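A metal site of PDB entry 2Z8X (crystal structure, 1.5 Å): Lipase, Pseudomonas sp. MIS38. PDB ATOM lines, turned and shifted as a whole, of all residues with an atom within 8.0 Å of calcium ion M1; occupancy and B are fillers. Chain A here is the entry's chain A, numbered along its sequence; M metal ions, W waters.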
ATOM      1  N   VAL A 522       4.651  18.101 -37.576  1.00  0.00           N
ATOM      2  CA  VAL A 522       5.280  16.840 -37.929  1.00  0.00           C
ATOM      3  C   VAL A 522       6.771  16.843 -37.603  1.00  0.00           C
ATOM      4  O   VAL A 522       7.433  15.802 -37.659  1.00  0.00           O
ATOM      5  CB  VAL A 522       5.081  16.504 -39.436  1.00  0.00           C
ATOM      6  CG1 VAL A 522       3.598  16.419 -39.758  1.00  0.00           C
ATOM      7  CG2 VAL A 522       5.765  17.544 -40.321  1.00  0.00           C
ATOM      8  N   GLY A 523       7.304  18.023 -37.296  1.00  0.00           N
ATOM      9  CA  GLY A 523       8.705  18.187 -36.974  1.00  0.00           C
ATOM     10  C   GLY A 523       9.001  17.942 -35.512  1.00  0.00           C
ATOM     11  O   GLY A 523       8.092  17.673 -34.732  1.00  0.00           O
ATOM     12  N   ASN A 524      10.274  18.049 -35.159  1.00  0.00           N
ATOM     13  CA  ASN A 524      10.749  17.830 -33.815  1.00  0.00           C
ATOM     14  C   ASN A 524      10.611  19.118 -33.035  1.00  0.00           C
ATOM     15  O   ASN A 524      11.357  20.079 -33.242  1.00  0.00           O
ATOM     16  CB  ASN A 524      12.204  17.369 -33.838  1.00  0.00           C
ATOM     17  CG  ASN A 524      12.391  16.042 -34.568  1.00  0.00           C
ATOM     18  OD1 ASN A 524      11.440  15.334 -34.874  1.00  0.00           O
ATOM     19  ND2 ASN A 524      13.653  15.702 -34.836  1.00  0.00           N
ATOM     20  N   SER A 538       1.664  16.633 -29.706  1.00  0.00           N
ATOM     21  CA  SER A 538       2.909  16.342 -30.409  1.00  0.00           C
ATOM     22  C   SER A 538       2.861  16.706 -31.900  1.00  0.00           C
ATOM     23  O   SER A 538       3.753  17.395 -32.420  1.00  0.00           O
ATOM     24  CB  SER A 538       3.267  14.857 -30.251  1.00  0.00           C
ATOM     25  OG  SER A 538       4.193  14.445 -31.251  1.00  0.00           O
ATOM     26  N   GLY A 539       1.840  16.220 -32.588  1.00  0.00           N
ATOM     27  CA  GLY A 539       1.730  16.455 -34.025  1.00  0.00           C
ATOM     28  C   GLY A 539       2.605  15.540 -34.888  1.00  0.00           C
ATOM     29  O   GLY A 539       2.547  15.625 -36.114  1.00  0.00           O
ATOM     30  N   GLY A 540       3.392  14.674 -34.261  1.00  0.00           N
ATOM     31  CA  GLY A 540       4.345  13.809 -34.976  1.00  0.00           C
ATOM     32  C   GLY A 540       5.781  14.196 -34.665  1.00  0.00           C
ATOM     33  O   GLY A 540       6.035  15.188 -33.990  1.00  0.00           O
ATOM     34  N   GLY A 541       6.728  13.400 -35.141  1.00  0.00           N
ATOM     35  CA  GLY A 541       8.139  13.704 -34.960  1.00  0.00           C
ATOM     36  C   GLY A 541       8.662  13.211 -33.627  1.00  0.00           C
ATOM     37  O   GLY A 541       7.967  12.480 -32.905  1.00  0.00           O
ATOM     38  N   ALA A 542       9.892  13.595 -33.317  1.00  0.00           N
ATOM     39  CA  ALA A 542      10.535  13.258 -32.051  1.00  0.00           C
ATOM     40  C   ALA A 542      10.565  14.516 -31.200  1.00  0.00           C
ATOM     41  O   ALA A 542      11.412  15.398 -31.375  1.00  0.00           O
ATOM     42  CB  ALA A 542      11.944  12.713 -32.298  1.00  0.00           C
ATOM     43  N   ASP A 543       9.590  14.609 -30.291  1.00  0.00           N
ATOM     44  CA  ASP A 543       9.334  15.815 -29.521  1.00  0.00           C
ATOM     45  C   ASP A 543       9.847  15.718 -28.096  1.00  0.00           C
ATOM     46  O   ASP A 543       9.970  14.627 -27.537  1.00  0.00           O
ATOM     47  CB  ASP A 543       7.825  16.110 -29.496  1.00  0.00           C
ATOM     48  CG  ASP A 543       7.261  16.474 -30.877  1.00  0.00           C
ATOM     49  OD1 ASP A 543       8.018  16.957 -31.741  1.00  0.00           O
ATOM     50  OD2 ASP A 543       6.048  16.315 -31.082  1.00  0.00           O
ATOM     51  N   THR A 544      10.113  16.881 -27.503  1.00  0.00           N
ATOM     52  CA  THR A 544      10.563  17.010 -26.133  1.00  0.00           C
ATOM     53  C   THR A 544       9.560  17.883 -25.400  1.00  0.00           C
ATOM     54  O   THR A 544       9.137  18.892 -25.934  1.00  0.00           O
ATOM     55  CB  THR A 544      11.959  17.689 -26.093  1.00  0.00           C
ATOM     56  OG1 THR A 544      12.876  16.927 -26.884  1.00  0.00           O
ATOM     57  CG2 THR A 544      12.465  17.814 -24.668  1.00  0.00           C
ATOM     58  N   PHE A 545       9.152  17.452 -24.201  1.00  0.00           N
ATOM     59  CA  PHE A 545       8.245  18.237 -23.358  1.00  0.00           C
ATOM     60  C   PHE A 545       9.002  18.546 -22.076  1.00  0.00           C
ATOM     61  O   PHE A 545       9.435  17.632 -21.374  1.00  0.00           O
ATOM     62  CB  PHE A 545       6.972  17.441 -23.055  1.00  0.00           C
ATOM     63  CG  PHE A 545       6.197  17.028 -24.292  1.00  0.00           C
ATOM     64  CD1 PHE A 545       5.061  17.744 -24.693  1.00  0.00           C
ATOM     65  CD2 PHE A 545       6.608  15.938 -25.052  1.00  0.00           C
ATOM     66  CE1 PHE A 545       4.343  17.365 -25.839  1.00  0.00           C
ATOM     67  CE2 PHE A 545       5.896  15.539 -26.195  1.00  0.00           C
ATOM     68  CZ  PHE A 545       4.774  16.272 -26.588  1.00  0.00           C
ATOM     69  N   GLY A 558      -0.548  12.604 -27.972  1.00  0.00           N
ATOM     70  CA  GLY A 558       0.250  12.072 -29.068  1.00  0.00           C
ATOM     71  C   GLY A 558       1.647  11.639 -28.688  1.00  0.00           C
ATOM     72  O   GLY A 558       2.516  11.549 -29.565  1.00  0.00           O
ATOM     73  N   PHE A 559       1.885  11.388 -27.397  1.00  0.00           N
ATOM     74  CA  PHE A 559       3.195  10.965 -26.916  1.00  0.00           C
ATOM     75  C   PHE A 559       3.505   9.556 -27.417  1.00  0.00           C
ATOM     76  O   PHE A 559       2.705   8.634 -27.251  1.00  0.00           O
ATOM     77  CB  PHE A 559       3.267  11.010 -25.382  1.00  0.00           C
ATOM     78  CG  PHE A 559       4.637  10.728 -24.807  1.00  0.00           C
ATOM     79  CD1 PHE A 559       5.568  11.755 -24.657  1.00  0.00           C
ATOM     80  CD2 PHE A 559       4.989   9.441 -24.398  1.00  0.00           C
ATOM     81  CE1 PHE A 559       6.833  11.507 -24.118  1.00  0.00           C
ATOM     82  CE2 PHE A 559       6.258   9.185 -23.858  1.00  0.00           C
ATOM     83  CZ  PHE A 559       7.177  10.218 -23.714  1.00  0.00           C
ATOM     84  N   THR A 560       4.658   9.414 -28.066  1.00  0.00           N
ATOM     85  CA  THR A 560       5.097   8.101 -28.561  1.00  0.00           C
ATOM     86  C   THR A 560       6.508   7.794 -28.021  1.00  0.00           C
ATOM     87  O   THR A 560       7.136   8.655 -27.390  1.00  0.00           O
ATOM     88  CB  THR A 560       5.098   7.991 -30.113  1.00  0.00           C
ATOM     89  OG1 THR A 560       6.204   8.715 -30.649  1.00  0.00           O
ATOM     90  CG2 THR A 560       3.774   8.496 -30.716  1.00  0.00           C
ATOM     91  N   SER A 561       7.001   6.587 -28.301  1.00  0.00           N
ATOM     92  CA  SER A 561       8.267   6.103 -27.720  1.00  0.00           C
ATOM     93  C   SER A 561       9.495   6.954 -28.047  1.00  0.00           C
ATOM     94  O   SER A 561      10.465   6.958 -27.281  1.00  0.00           O
ATOM     95  CB  SER A 561       8.506   4.644 -28.123  1.00  0.00           C
ATOM     96  OG  SER A 561       7.506   3.835 -27.540  1.00  0.00           O
ATOM     97  N   ASN A 562       9.458   7.657 -29.183  1.00  0.00           N
ATOM     98  CA  ASN A 562      10.616   8.471 -29.596  1.00  0.00           C
ATOM     99  C   ASN A 562      10.554   9.894 -29.047  1.00  0.00           C
ATOM    100  O   ASN A 562      11.419  10.703 -29.373  1.00  0.00           O
ATOM    101  CB  ASN A 562      10.819   8.462 -31.124  1.00  0.00           C
ATOM    102  CG  ASN A 562       9.800   9.327 -31.882  1.00  0.00           C
ATOM    103  OD1 ASN A 562       8.738   9.667 -31.363  1.00  0.00           O
ATOM    104  ND2 ASN A 562      10.123   9.648 -33.131  1.00  0.00           N
ATOM    105  N   ASP A 563       9.545  10.172 -28.235  1.00  0.00           N
ATOM    106  CA  ASP A 563       9.421  11.457 -27.562  1.00  0.00           C
ATOM    107  C   ASP A 563      10.012  11.394 -26.149  1.00  0.00           C
ATOM    108  O   ASP A 563      10.313  10.312 -25.628  1.00  0.00           O
ATOM    109  CB  ASP A 563       7.969  11.922 -27.525  1.00  0.00           C
ATOM    110  CG  ASP A 563       7.341  11.936 -28.902  1.00  0.00           C
ATOM    111  OD1 ASP A 563       7.994  12.413 -29.858  1.00  0.00           O
ATOM    112  OD2 ASP A 563       6.191  11.479 -29.042  1.00  0.00           O
ATOM    113  N   LYS A 564      10.204  12.555 -25.553  1.00  0.00           N
ATOM    114  CA  LYS A 564      10.840  12.626 -24.251  1.00  0.00           C
ATOM    115  C   LYS A 564      10.158  13.652 -23.357  1.00  0.00           C
ATOM    116  O   LYS A 564       9.828  14.758 -23.802  1.00  0.00           O
ATOM    117  CB  LYS A 564      12.320  12.979 -24.420  1.00  0.00           C
ATOM    118  CG  LYS A 564      13.133  12.912 -23.135  1.00  0.00           C
ATOM    119  CD  LYS A 564      14.637  13.013 -23.398  1.00  0.00           C
ATOM    120  CE  LYS A 564      15.018  14.339 -24.025  1.00  0.00           C
ATOM    121  NZ  LYS A 564      16.463  14.383 -24.379  1.00  0.00           N
HETATM  122 CA    CA M   1       6.804  10.971 -31.482  1.00  0.00          CA
HETATM  123 CA    CA M   2       6.073  17.404 -33.338  1.00  0.00          CA
HETATM  124  O   HOH W   1       6.388   9.877 -33.537  1.00  0.00           O
HETATM  125  O   HOH W   2       4.725  11.919 -31.988  1.00  0.00           O
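N of Asp 543 lies close to OD1 of Asp 563.
Of the 18 residues printed, 4 come within 4 Å of calcium ion M1.
The nearest printed residue that does not touch calcium ion M1 is Ser 538 (4.4 Å).
Calcium ion M1 is bound by OD1 of Asn 562.
Water W2 binds calcium ion M1.
Water W1 binds calcium ion M1 (2.4 Å).
O of Gly 541 is bound to calcium ion M1 (2.4 Å).
Calcium ion M1 is bound by OD1 of Asp 563 (2.5 Å).
Calcium ion M1 is bound by OG1 of Thr 560.
Calcium ion M1 is bound by the side-chain carboxylate (OD2) of Asp 563.
Water W2 lies within hydrogen-bond range of OG of Ser 538 (2.7 Å) and O of Gly 558 (3.3 Å).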
